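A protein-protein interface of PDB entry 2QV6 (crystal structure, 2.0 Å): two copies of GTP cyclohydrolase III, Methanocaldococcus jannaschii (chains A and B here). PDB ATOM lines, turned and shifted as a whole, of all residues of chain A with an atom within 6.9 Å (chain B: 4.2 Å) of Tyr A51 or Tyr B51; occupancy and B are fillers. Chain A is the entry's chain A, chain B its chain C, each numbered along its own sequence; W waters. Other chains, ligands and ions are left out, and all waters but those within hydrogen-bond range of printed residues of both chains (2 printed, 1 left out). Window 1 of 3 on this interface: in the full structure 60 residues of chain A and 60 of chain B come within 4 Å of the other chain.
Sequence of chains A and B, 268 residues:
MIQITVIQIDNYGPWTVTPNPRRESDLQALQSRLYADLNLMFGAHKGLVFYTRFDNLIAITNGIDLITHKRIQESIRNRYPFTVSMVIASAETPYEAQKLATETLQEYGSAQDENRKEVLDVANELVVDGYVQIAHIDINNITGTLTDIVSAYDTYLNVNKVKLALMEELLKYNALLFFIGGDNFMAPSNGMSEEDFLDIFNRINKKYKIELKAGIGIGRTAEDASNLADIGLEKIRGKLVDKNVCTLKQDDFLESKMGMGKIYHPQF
Hydrophobic or aromatic side chains of chain A within 4 Å of the printed part of chain B: Tyr A51, Phe A54 and Tyr A156. Hydrophobic or aromatic side chains of chain B within 4 Å of the printed part of chain A: Tyr B35, Tyr B51, Phe B54 and Phe B179. Among the printed residues, no Asp or Glu carboxylate lies within 4 Å of a Lys or Arg side-chain nitrogen of the other chain.
The side-chain hydroxyl (OG) of Ser A32 lies within hydrogen-bond range of the backbone carbonyl oxygen (O) of Gln A28 (2.6 Å). The side-chain carboxylate (OD1) of Asp A55 is in salt-bridge range of the guanidinium group (NH1) of Arg A53. The side-chain amide nitrogen (ND2) of Asn A56 sits close to the guanidinium group (NH2) of Arg A53. The side-chain amide nitrogen (ND2) of Asn A160 is in hydrogen-bond range of the backbone carbonyl oxygen (O) of Tyr A156, 2.7 Å away. The backbone carbonyl oxygen of Phe B50 is in hydrogen-bond range of the side-chain hydroxyl of Thr B52, at 3.0 Å. ND2 of Asn B56 sits close to NH2 of Arg B53 (3.1 Å).
OG of Ser A32 touches CD2 of Tyr B35, 3.0 Å away. Tyr B51 touches Tyr A51. Tyr A51 touches Phe B54 (CE2 to CE2, 3.7 Å). CA of Arg A53 touches CE2 of Phe B179, at 3.9 Å. Tyr B51 touches Phe A54. Tyr A156 touches Thr B52. Arg B53 touches Tyr A156 (CD to CA, 3.9 Å). Asn A160 touches Lys B163 (OD1 to CE, 3.6 Å). NZ of Lys B163 touches NZ of Lys A163, at 3.8 Å. Gly A181 touches Arg B53 (CA to O, 3.4 Å).
Printed residues of chain B within 4 Å of Gln A28: Tyr B35. Of chain B, only Tyr B51 (3.8 Å) and Phe B54 (3.7 Å) come within 4 Å of Tyr A51. Thr A52 touches none of the printed residues of chain B. Asp A55 touches none of the printed residues of chain B. Printed residues of chain B within 4 Å of Gly A181: Arg B53. Of the printed residues of chain A, Tyr B35 touches Gln A28 and Ser A32. Tyr B51 touches just these residues of chain A: Tyr A51 (3.8 Å) and Phe A54 (3.9 Å).
Water W2 lies within hydrogen-bond range of NZ of Lys A163, NZ of Lys B163, OH of Tyr A51 and OH of Tyr B51. Water W1 bridges OH of Tyr A156 and N of Phe B179.
Tyr A51 touches its own counterpart, Tyr B51. Tyr A51 touches Phe B54, and with the chains exchanged Phe A54 touches Tyr B51. Arg A53 touches Phe B179, but with the chains exchanged Phe A179 does not touch Arg B53 (4.1 Å). Lys A163 touches its own counterpart, Lys B163. Positions printed for both chains: 35, 50, 51, 52, 53, 54, 56, 57, 163 and 179. Of the 11 pairs that touch across the chains among the printed residues, 4 have their exchanged pair printed and touching as well.
The side-chain hydroxyl (OH) of Tyr B35 is in hydrogen-bond range of the side-chain amide nitrogen (NE2) of Gln A28, at 2.6 Å.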
ATOM      1  N   GLN A  28      31.320 -25.730  -3.204  1.00  0.00           N
ATOM      2  CA  GLN A  28      30.967 -24.468  -3.856  1.00  0.00           C
ATOM      3  C   GLN A  28      30.891 -24.573  -5.382  1.00  0.00           C
ATOM      4  O   GLN A  28      29.947 -24.021  -6.003  1.00  0.00           O
ATOM      5  CB  GLN A  28      31.939 -23.357  -3.452  1.00  0.00           C
ATOM      6  CG  GLN A  28      31.774 -22.895  -1.980  1.00  0.00           C
ATOM      7  CD  GLN A  28      30.324 -22.579  -1.589  1.00  0.00           C
ATOM      8  OE1 GLN A  28      29.723 -23.320  -0.829  1.00  0.00           O
ATOM      9  NE2 GLN A  28      29.783 -21.476  -2.095  1.00  0.00           N
ATOM     10  N   SER A  32      27.420 -24.217  -7.583  1.00  0.00           N
ATOM     11  CA  SER A  32      27.359 -23.202  -8.641  1.00  0.00           C
ATOM     12  C   SER A  32      27.169 -23.816 -10.009  1.00  0.00           C
ATOM     13  O   SER A  32      26.456 -23.277 -10.847  1.00  0.00           O
ATOM     14  CB  SER A  32      28.663 -22.398  -8.689  1.00  0.00           C
ATOM     15  OG  SER A  32      29.033 -22.000  -7.403  1.00  0.00           O
ATOM     16  N   TYR A  35      23.498 -24.789 -10.369  1.00  0.00           N
ATOM     17  CA  TYR A  35      22.774 -23.540 -10.629  1.00  0.00           C
ATOM     18  C   TYR A  35      22.940 -23.051 -12.062  1.00  0.00           C
ATOM     19  O   TYR A  35      21.951 -22.619 -12.700  1.00  0.00           O
ATOM     20  CB  TYR A  35      23.212 -22.452  -9.613  1.00  0.00           C
ATOM     21  CG  TYR A  35      22.576 -21.101  -9.779  1.00  0.00           C
ATOM     22  CD1 TYR A  35      21.192 -20.968  -9.897  1.00  0.00           C
ATOM     23  CD2 TYR A  35      23.338 -19.946  -9.787  1.00  0.00           C
ATOM     24  CE1 TYR A  35      20.604 -19.734 -10.063  1.00  0.00           C
ATOM     25  CE2 TYR A  35      22.742 -18.671  -9.904  1.00  0.00           C
ATOM     26  CZ  TYR A  35      21.370 -18.577 -10.051  1.00  0.00           C
ATOM     27  OH  TYR A  35      20.732 -17.356 -10.196  1.00  0.00           O
ATOM     28  N   ASN A  39      19.863 -22.862 -15.057  1.00  0.00           N
ATOM     29  CA  ASN A  39      19.579 -21.678 -15.883  1.00  0.00           C
ATOM     30  C   ASN A  39      19.814 -21.870 -17.384  1.00  0.00           C
ATOM     31  O   ASN A  39      19.084 -21.308 -18.175  1.00  0.00           O
ATOM     32  CB  ASN A  39      20.347 -20.419 -15.410  1.00  0.00           C
ATOM     33  CG  ASN A  39      19.533 -19.543 -14.491  1.00  0.00           C
ATOM     34  OD1 ASN A  39      19.965 -19.218 -13.400  1.00  0.00           O
ATOM     35  ND2 ASN A  39      18.299 -19.217 -14.895  1.00  0.00           N
ATOM     36  N   VAL A  49      15.833 -19.178 -13.196  1.00  0.00           N
ATOM     37  CA  VAL A  49      16.031 -19.842 -11.916  1.00  0.00           C
ATOM     38  C   VAL A  49      16.842 -18.878 -11.030  1.00  0.00           C
ATOM     39  O   VAL A  49      17.771 -18.244 -11.507  1.00  0.00           O
ATOM     40  CB  VAL A  49      16.869 -21.202 -12.047  1.00  0.00           C
ATOM     41  CG1 VAL A  49      16.932 -21.964 -10.711  1.00  0.00           C
ATOM     42  CG2 VAL A  49      16.323 -22.119 -13.135  1.00  0.00           C
ATOM     43  N   PHE A  50      16.463 -18.772  -9.756  1.00  0.00           N
ATOM     44  CA  PHE A  50      17.216 -18.007  -8.741  1.00  0.00           C
ATOM     45  C   PHE A  50      17.794 -18.956  -7.740  1.00  0.00           C
ATOM     46  O   PHE A  50      17.196 -19.979  -7.450  1.00  0.00           O
ATOM     47  CB  PHE A  50      16.302 -17.011  -8.039  1.00  0.00           C
ATOM     48  CG  PHE A  50      15.540 -16.130  -8.988  1.00  0.00           C
ATOM     49  CD1 PHE A  50      16.127 -15.013  -9.542  1.00  0.00           C
ATOM     50  CD2 PHE A  50      14.244 -16.423  -9.329  1.00  0.00           C
ATOM     51  CE1 PHE A  50      15.415 -14.197 -10.425  1.00  0.00           C
ATOM     52  CE2 PHE A  50      13.538 -15.611 -10.217  1.00  0.00           C
ATOM     53  CZ  PHE A  50      14.110 -14.510 -10.754  1.00  0.00           C
ATOM     54  N   TYR A  51      18.968 -18.636  -7.200  1.00  0.00           N
ATOM     55  CA  TYR A  51      19.720 -19.635  -6.467  1.00  0.00           C
ATOM     56  C   TYR A  51      19.180 -19.944  -5.072  1.00  0.00           C
ATOM     57  O   TYR A  51      19.307 -21.090  -4.607  1.00  0.00           O
ATOM     58  CB  TYR A  51      21.231 -19.271  -6.430  1.00  0.00           C
ATOM     59  CG  TYR A  51      21.624 -18.007  -5.700  1.00  0.00           C
ATOM     60  CD1 TYR A  51      21.610 -17.935  -4.309  1.00  0.00           C
ATOM     61  CD2 TYR A  51      22.121 -16.918  -6.394  1.00  0.00           C
ATOM     62  CE1 TYR A  51      21.983 -16.792  -3.660  1.00  0.00           C
ATOM     63  CE2 TYR A  51      22.526 -15.783  -5.743  1.00  0.00           C
ATOM     64  CZ  TYR A  51      22.445 -15.716  -4.389  1.00  0.00           C
ATOM     65  OH  TYR A  51      22.844 -14.549  -3.763  1.00  0.00           O
ATOM     66  N   THR A  52      18.633 -18.924  -4.400  1.00  0.00           N
ATOM     67  CA  THR A  52      17.896 -19.078  -3.179  1.00  0.00           C
ATOM     68  C   THR A  52      18.848 -19.558  -2.066  1.00  0.00           C
ATOM     69  O   THR A  52      19.685 -18.767  -1.630  1.00  0.00           O
ATOM     70  CB  THR A  52      16.650 -19.950  -3.443  1.00  0.00           C
ATOM     71  OG1 THR A  52      15.979 -19.424  -4.594  1.00  0.00           O
ATOM     72  CG2 THR A  52      15.685 -19.962  -2.255  1.00  0.00           C
ATOM     73  N   ARG A  53      18.753 -20.832  -1.662  1.00  0.00           N
ATOM     74  CA  ARG A  53      19.643 -21.419  -0.665  1.00  0.00           C
ATOM     75  C   ARG A  53      20.620 -22.459  -1.219  1.00  0.00           C
ATOM     76  O   ARG A  53      21.370 -23.055  -0.452  1.00  0.00           O
ATOM     77  CB  ARG A  53      18.796 -22.039   0.450  1.00  0.00           C
ATOM     78  CG  ARG A  53      18.076 -20.985   1.254  1.00  0.00           C
ATOM     79  CD  ARG A  53      17.595 -21.476   2.591  1.00  0.00           C
ATOM     80  NE  ARG A  53      16.704 -22.639   2.489  1.00  0.00           N
ATOM     81  CZ  ARG A  53      16.954 -23.802   3.068  1.00  0.00           C
ATOM     82  NH1 ARG A  53      18.031 -23.976   3.829  1.00  0.00           N
ATOM     83  NH2 ARG A  53      16.097 -24.790   2.943  1.00  0.00           N
ATOM     84  N   PHE A  54      20.593 -22.669  -2.538  1.00  0.00           N
ATOM     85  CA  PHE A  54      21.455 -23.639  -3.252  1.00  0.00           C
ATOM     86  C   PHE A  54      21.014 -25.101  -3.194  1.00  0.00           C
ATOM     87  O   PHE A  54      20.860 -25.725  -4.249  1.00  0.00           O
ATOM     88  CB  PHE A  54      22.925 -23.485  -2.880  1.00  0.00           C
ATOM     89  CG  PHE A  54      23.537 -22.231  -3.411  1.00  0.00           C
ATOM     90  CD1 PHE A  54      23.833 -22.116  -4.757  1.00  0.00           C
ATOM     91  CD2 PHE A  54      23.807 -21.147  -2.567  1.00  0.00           C
ATOM     92  CE1 PHE A  54      24.393 -20.957  -5.249  1.00  0.00           C
ATOM     93  CE2 PHE A  54      24.408 -19.985  -3.063  1.00  0.00           C
ATOM     94  CZ  PHE A  54      24.689 -19.891  -4.394  1.00  0.00           C
ATOM     95  N   ASP A  55      20.737 -25.621  -1.999  1.00  0.00           N
ATOM     96  CA  ASP A  55      20.137 -26.928  -1.867  1.00  0.00           C
ATOM     97  C   ASP A  55      18.636 -26.890  -2.146  1.00  0.00           C
ATOM     98  O   ASP A  55      18.067 -27.941  -2.336  1.00  0.00           O
ATOM     99  CB  ASP A  55      20.381 -27.538  -0.505  1.00  0.00           C
ATOM    100  CG  ASP A  55      19.704 -26.782   0.653  1.00  0.00           C
ATOM    101  OD1 ASP A  55      19.365 -25.578   0.528  1.00  0.00           O
ATOM    102  OD2 ASP A  55      19.547 -27.425   1.727  1.00  0.00           O
ATOM    103  N   ASN A  56      18.034 -25.695  -2.138  1.00  0.00           N
ATOM    104  CA  ASN A  56      16.619 -25.450  -2.568  1.00  0.00           C
ATOM    105  C   ASN A  56      16.595 -24.253  -3.504  1.00  0.00           C
ATOM    106  O   ASN A  56      17.190 -23.239  -3.174  1.00  0.00           O
ATOM    107  CB  ASN A  56      15.743 -25.088  -1.342  1.00  0.00           C
ATOM    108  CG  ASN A  56      15.247 -26.296  -0.560  1.00  0.00           C
ATOM    109  OD1 ASN A  56      14.159 -26.842  -0.836  1.00  0.00           O
ATOM    110  ND2 ASN A  56      15.998 -26.687   0.456  1.00  0.00           N
ATOM    111  N   LEU A  57      15.884 -24.321  -4.640  1.00  0.00           N
ATOM    112  CA  LEU A  57      15.850 -23.242  -5.618  1.00  0.00           C
ATOM    113  C   LEU A  57      14.410 -22.950  -6.122  1.00  0.00           C
ATOM    114  O   LEU A  57      13.521 -23.823  -6.063  1.00  0.00           O
ATOM    115  CB  LEU A  57      16.771 -23.580  -6.797  1.00  0.00           C
ATOM    116  CG  LEU A  57      18.215 -24.023  -6.491  1.00  0.00           C
ATOM    117  CD1 LEU A  57      18.387 -25.542  -6.435  1.00  0.00           C
ATOM    118  CD2 LEU A  57      19.222 -23.446  -7.462  1.00  0.00           C
ATOM    119  N   ILE A  58      14.190 -21.712  -6.586  1.00  0.00           N
ATOM    120  CA  ILE A  58      12.885 -21.282  -7.137  1.00  0.00           C
ATOM    121  C   ILE A  58      13.096 -20.832  -8.583  1.00  0.00           C
ATOM    122  O   ILE A  58      14.091 -20.161  -8.902  1.00  0.00           O
ATOM    123  CB  ILE A  58      12.206 -20.181  -6.287  1.00  0.00           C
ATOM    124  CG1 ILE A  58      11.845 -20.747  -4.906  1.00  0.00           C
ATOM    125  CG2 ILE A  58      10.908 -19.658  -6.983  1.00  0.00           C
ATOM    126  CD1 ILE A  58      11.848 -19.760  -3.774  1.00  0.00           C
ATOM    127  N   TYR A 156      29.463  -4.895   0.356  1.00  0.00           N
ATOM    128  CA  TYR A 156      28.708  -6.169   0.475  1.00  0.00           C
ATOM    129  C   TYR A 156      27.722  -6.160   1.659  1.00  0.00           C
ATOM    130  O   TYR A 156      26.576  -6.612   1.562  1.00  0.00           O
ATOM    131  CB  TYR A 156      29.734  -7.327   0.528  1.00  0.00           C
ATOM    132  CG  TYR A 156      29.307  -8.603   1.196  1.00  0.00           C
ATOM    133  CD1 TYR A 156      28.698  -9.609   0.480  1.00  0.00           C
ATOM    134  CD2 TYR A 156      29.573  -8.830   2.536  1.00  0.00           C
ATOM    135  CE1 TYR A 156      28.315 -10.820   1.082  1.00  0.00           C
ATOM    136  CE2 TYR A 156      29.195 -10.033   3.159  1.00  0.00           C
ATOM    137  CZ  TYR A 156      28.579 -11.031   2.427  1.00  0.00           C
ATOM    138  OH  TYR A 156      28.212 -12.211   3.031  1.00  0.00           O
ATOM    139  N   ASN A 160      23.558  -6.196   1.301  1.00  0.00           N
ATOM    140  CA  ASN A 160      22.761  -7.165   2.068  1.00  0.00           C
ATOM    141  C   ASN A 160      21.685  -6.565   3.009  1.00  0.00           C
ATOM    142  O   ASN A 160      20.593  -7.147   3.157  1.00  0.00           O
ATOM    143  CB  ASN A 160      23.686  -8.117   2.820  1.00  0.00           C
ATOM    144  CG  ASN A 160      24.240  -9.217   1.911  1.00  0.00           C
ATOM    145  OD1 ASN A 160      23.540 -10.162   1.598  1.00  0.00           O
ATOM    146  ND2 ASN A 160      25.483  -9.087   1.491  1.00  0.00           N
ATOM    147  N   LYS A 163      18.846  -5.543   0.662  1.00  0.00           N
ATOM    148  CA  LYS A 163      18.221  -6.796   0.223  1.00  0.00           C
ATOM    149  C   LYS A 163      17.170  -7.314   1.176  1.00  0.00           C
ATOM    150  O   LYS A 163      16.096  -7.746   0.757  1.00  0.00           O
ATOM    151  CB  LYS A 163      19.299  -7.855   0.093  1.00  0.00           C
ATOM    152  CG  LYS A 163      18.834  -9.240  -0.253  1.00  0.00           C
ATOM    153  CD  LYS A 163      20.039  -9.987  -0.694  1.00  0.00           C
ATOM    154  CE  LYS A 163      19.926 -11.458  -0.528  1.00  0.00           C
ATOM    155  NZ  LYS A 163      21.320 -12.043  -0.783  1.00  0.00           N
ATOM    156  N   PHE A 178      15.043 -11.553  -4.990  1.00  0.00           N
ATOM    157  CA  PHE A 178      16.270 -12.358  -5.175  1.00  0.00           C
ATOM    158  C   PHE A 178      17.467 -11.511  -5.614  1.00  0.00           C
ATOM    159  O   PHE A 178      17.355 -10.697  -6.511  1.00  0.00           O
ATOM    160  CB  PHE A 178      16.017 -13.459  -6.218  1.00  0.00           C
ATOM    161  CG  PHE A 178      14.913 -14.417  -5.836  1.00  0.00           C
ATOM    162  CD1 PHE A 178      15.137 -15.422  -4.928  1.00  0.00           C
ATOM    163  CD2 PHE A 178      13.654 -14.313  -6.401  1.00  0.00           C
ATOM    164  CE1 PHE A 178      14.143 -16.303  -4.571  1.00  0.00           C
ATOM    165  CE2 PHE A 178      12.649 -15.204  -6.065  1.00  0.00           C
ATOM    166  CZ  PHE A 178      12.875 -16.187  -5.154  1.00  0.00           C
ATOM    167  N   PHE A 179      18.631 -11.719  -5.001  1.00  0.00           N
ATOM    168  CA  PHE A 179      19.855 -11.059  -5.466  1.00  0.00           C
ATOM    169  C   PHE A 179      20.362 -11.693  -6.770  1.00  0.00           C
ATOM    170  O   PHE A 179      20.359 -12.911  -6.894  1.00  0.00           O
ATOM    171  CB  PHE A 179      20.942 -11.189  -4.392  1.00  0.00           C
ATOM    172  CG  PHE A 179      22.147 -10.357  -4.655  1.00  0.00           C
ATOM    173  CD1 PHE A 179      22.032  -9.034  -5.052  1.00  0.00           C
ATOM    174  CD2 PHE A 179      23.420 -10.881  -4.474  1.00  0.00           C
ATOM    175  CE1 PHE A 179      23.158  -8.246  -5.282  1.00  0.00           C
ATOM    176  CE2 PHE A 179      24.526 -10.098  -4.710  1.00  0.00           C
ATOM    177  CZ  PHE A 179      24.393  -8.781  -5.077  1.00  0.00           C
ATOM    178  N   ILE A 180      20.788 -10.888  -7.744  1.00  0.00           N
ATOM    179  CA  ILE A 180      21.339 -11.426  -9.001  1.00  0.00           C
ATOM    180  C   ILE A 180      22.769 -10.959  -9.329  1.00  0.00           C
ATOM    181  O   ILE A 180      23.332 -11.297 -10.369  1.00  0.00           O
ATOM    182  CB  ILE A 180      20.308 -11.305 -10.180  1.00  0.00           C
ATOM    183  CG1 ILE A 180      19.792  -9.877 -10.351  1.00  0.00           C
ATOM    184  CG2 ILE A 180      19.121 -12.215  -9.888  1.00  0.00           C
ATOM    185  CD1 ILE A 180      19.692  -9.401 -11.803  1.00  0.00           C
ATOM    186  N   GLY A 181      23.404 -10.292  -8.367  1.00  0.00           N
ATOM    187  CA  GLY A 181      24.782  -9.868  -8.480  1.00  0.00           C
ATOM    188  C   GLY A 181      24.845  -8.365  -8.579  1.00  0.00           C
ATOM    189  O   GLY A 181      23.873  -7.694  -9.031  1.00  0.00           O
ATOM    190  N   TYR B  35      32.598 -18.267 -10.699  1.00  0.00           N
ATOM    191  CA  TYR B  35      32.757 -18.531  -9.263  1.00  0.00           C
ATOM    192  C   TYR B  35      33.263 -19.945  -9.013  1.00  0.00           C
ATOM    193  O   TYR B  35      34.118 -20.153  -8.161  1.00  0.00           O
ATOM    194  CB  TYR B  35      31.438 -18.295  -8.501  1.00  0.00           C
ATOM    195  CG  TYR B  35      31.445 -18.694  -7.035  1.00  0.00           C
ATOM    196  CD1 TYR B  35      32.439 -18.251  -6.185  1.00  0.00           C
ATOM    197  CD2 TYR B  35      30.431 -19.476  -6.491  1.00  0.00           C
ATOM    198  CE1 TYR B  35      32.458 -18.600  -4.872  1.00  0.00           C
ATOM    199  CE2 TYR B  35      30.418 -19.797  -5.150  1.00  0.00           C
ATOM    200  CZ  TYR B  35      31.446 -19.364  -4.344  1.00  0.00           C
ATOM    201  OH  TYR B  35      31.482 -19.666  -2.998  1.00  0.00           O
ATOM    202  N   PHE B  50      34.625 -16.859  -1.828  1.00  0.00           N
ATOM    203  CA  PHE B  50      33.252 -16.634  -1.439  1.00  0.00           C
ATOM    204  C   PHE B  50      32.602 -15.802  -2.496  1.00  0.00           C
ATOM    205  O   PHE B  50      33.190 -14.875  -2.983  1.00  0.00           O
ATOM    206  CB  PHE B  50      33.232 -15.933  -0.109  1.00  0.00           C
ATOM    207  CG  PHE B  50      33.910 -16.719   0.965  1.00  0.00           C
ATOM    208  CD1 PHE B  50      33.324 -17.856   1.475  1.00  0.00           C
ATOM    209  CD2 PHE B  50      35.161 -16.360   1.419  1.00  0.00           C
ATOM    210  CE1 PHE B  50      33.964 -18.618   2.464  1.00  0.00           C
ATOM    211  CE2 PHE B  50      35.788 -17.107   2.404  1.00  0.00           C
ATOM    212  CZ  PHE B  50      35.200 -18.231   2.909  1.00  0.00           C
ATOM    213  N   TYR B  51      31.371 -16.117  -2.866  1.00  0.00           N
ATOM    214  CA  TYR B  51      30.802 -15.423  -4.015  1.00  0.00           C
ATOM    215  C   TYR B  51      30.648 -13.906  -3.807  1.00  0.00           C
ATOM    216  O   TYR B  51      30.837 -13.128  -4.770  1.00  0.00           O
ATOM    217  CB  TYR B  51      29.523 -16.116  -4.479  1.00  0.00           C
ATOM    218  CG  TYR B  51      28.366 -16.145  -3.518  1.00  0.00           C
ATOM    219  CD1 TYR B  51      28.087 -17.283  -2.804  1.00  0.00           C
ATOM    220  CD2 TYR B  51      27.508 -15.050  -3.383  1.00  0.00           C
ATOM    221  CE1 TYR B  51      26.992 -17.339  -1.949  1.00  0.00           C
ATOM    222  CE2 TYR B  51      26.403 -15.100  -2.537  1.00  0.00           C
ATOM    223  CZ  TYR B  51      26.164 -16.254  -1.810  1.00  0.00           C
ATOM    224  OH  TYR B  51      25.070 -16.363  -0.944  1.00  0.00           O
ATOM    225  N   THR B  52      30.329 -13.491  -2.567  1.00  0.00           N
ATOM    226  CA  THR B  52      30.241 -12.069  -2.175  1.00  0.00           C
ATOM    227  C   THR B  52      29.177 -11.304  -3.006  1.00  0.00           C
ATOM    228  O   THR B  52      27.974 -11.481  -2.729  1.00  0.00           O
ATOM    229  CB  THR B  52      31.667 -11.433  -2.193  1.00  0.00           C
ATOM    230  OG1 THR B  52      32.551 -12.307  -1.477  1.00  0.00           O
ATOM    231  CG2 THR B  52      31.698 -10.037  -1.539  1.00  0.00           C
ATOM    232  N   ARG B  53      29.581 -10.494  -3.998  1.00  0.00           N
ATOM    233  CA  ARG B  53      28.612  -9.846  -4.928  1.00  0.00           C
ATOM    234  C   ARG B  53      28.663 -10.329  -6.383  1.00  0.00           C
ATOM    235  O   ARG B  53      27.967  -9.764  -7.260  1.00  0.00           O
ATOM    236  CB  ARG B  53      28.775  -8.329  -4.885  1.00  0.00           C
ATOM    237  CG  ARG B  53      28.700  -7.787  -3.467  1.00  0.00           C
ATOM    238  CD  ARG B  53      28.331  -6.325  -3.425  1.00  0.00           C
ATOM    239  NE  ARG B  53      29.433  -5.487  -3.894  1.00  0.00           N
ATOM    240  CZ  ARG B  53      29.376  -4.687  -4.958  1.00  0.00           C
ATOM    241  NH1 ARG B  53      28.248  -4.538  -5.666  1.00  0.00           N
ATOM    242  NH2 ARG B  53      30.431  -3.976  -5.287  1.00  0.00           N
ATOM    243  N   PHE B  54      29.451 -11.376  -6.634  1.00  0.00           N
ATOM    244  CA  PHE B  54      29.643 -11.979  -7.963  1.00  0.00           C
ATOM    245  C   PHE B  54      30.486 -11.160  -8.945  1.00  0.00           C
ATOM    246  O   PHE B  54      31.354 -11.724  -9.571  1.00  0.00           O
ATOM    247  CB  PHE B  54      28.303 -12.381  -8.618  1.00  0.00           C
ATOM    248  CG  PHE B  54      27.635 -13.544  -7.970  1.00  0.00           C
ATOM    249  CD1 PHE B  54      28.099 -14.847  -8.201  1.00  0.00           C
ATOM    250  CD2 PHE B  54      26.529 -13.355  -7.144  1.00  0.00           C
ATOM    251  CE1 PHE B  54      27.466 -15.937  -7.611  1.00  0.00           C
ATOM    252  CE2 PHE B  54      25.892 -14.432  -6.560  1.00  0.00           C
ATOM    253  CZ  PHE B  54      26.356 -15.718  -6.788  1.00  0.00           C
ATOM    254  N   ASN B  56      32.320  -8.773  -7.576  1.00  0.00           N
ATOM    255  CA  ASN B  56      33.445  -8.596  -6.608  1.00  0.00           C
ATOM    256  C   ASN B  56      33.509  -9.807  -5.678  1.00  0.00           C
ATOM    257  O   ASN B  56      32.503 -10.154  -5.083  1.00  0.00           O
ATOM    258  CB  ASN B  56      33.218  -7.358  -5.715  1.00  0.00           C
ATOM    259  CG  ASN B  56      33.494  -6.025  -6.411  1.00  0.00           C
ATOM    260  OD1 ASN B  56      34.590  -5.486  -6.311  1.00  0.00           O
ATOM    261  ND2 ASN B  56      32.498  -5.486  -7.103  1.00  0.00           N
ATOM    262  N   LEU B  57      34.694 -10.402  -5.476  1.00  0.00           N
ATOM    263  CA  LEU B  57      34.854 -11.630  -4.684  1.00  0.00           C
ATOM    264  C   LEU B  57      36.020 -11.502  -3.714  1.00  0.00           C
ATOM    265  O   LEU B  57      36.979 -10.772  -3.988  1.00  0.00           O
ATOM    266  CB  LEU B  57      35.090 -12.842  -5.606  1.00  0.00           C
ATOM    267  CG  LEU B  57      34.062 -13.065  -6.728  1.00  0.00           C
ATOM    268  CD1 LEU B  57      34.461 -12.333  -8.012  1.00  0.00           C
ATOM    269  CD2 LEU B  57      33.832 -14.553  -7.014  1.00  0.00           C
ATOM    270  N   LYS B 163      21.611 -14.598   8.848  1.00  0.00           N
ATOM    271  CA  LYS B 163      22.803 -14.128   8.144  1.00  0.00           C
ATOM    272  C   LYS B 163      23.208 -12.684   8.450  1.00  0.00           C
ATOM    273  O   LYS B 163      24.378 -12.406   8.723  1.00  0.00           O
ATOM    274  CB  LYS B 163      22.609 -14.273   6.623  1.00  0.00           C
ATOM    275  CG  LYS B 163      23.776 -13.748   5.759  1.00  0.00           C
ATOM    276  CD  LYS B 163      23.745 -14.279   4.344  1.00  0.00           C
ATOM    277  CE  LYS B 163      23.235 -13.271   3.312  1.00  0.00           C
ATOM    278  NZ  LYS B 163      23.455 -13.800   1.883  1.00  0.00           N
ATOM    279  N   PHE B 179      27.536 -16.708   3.312  1.00  0.00           N
ATOM    280  CA  PHE B 179      26.612 -17.820   3.179  1.00  0.00           C
ATOM    281  C   PHE B 179      27.265 -18.858   2.265  1.00  0.00           C
ATOM    282  O   PHE B 179      27.899 -18.485   1.294  1.00  0.00           O
ATOM    283  CB  PHE B 179      25.320 -17.316   2.503  1.00  0.00           C
ATOM    284  CG  PHE B 179      24.257 -18.351   2.403  1.00  0.00           C
ATOM    285  CD1 PHE B 179      23.922 -19.125   3.509  1.00  0.00           C
ATOM    286  CD2 PHE B 179      23.543 -18.532   1.207  1.00  0.00           C
ATOM    287  CE1 PHE B 179      22.927 -20.082   3.419  1.00  0.00           C
ATOM    288  CE2 PHE B 179      22.575 -19.492   1.126  1.00  0.00           C
ATOM    289  CZ  PHE B 179      22.251 -20.248   2.220  1.00  0.00           C
HETATM  290  O   HOH W   1      27.339 -14.427   1.508  1.00  0.00           O
HETATM  291  O   HOH W   2      23.081 -14.017  -0.835  1.00  0.00           O
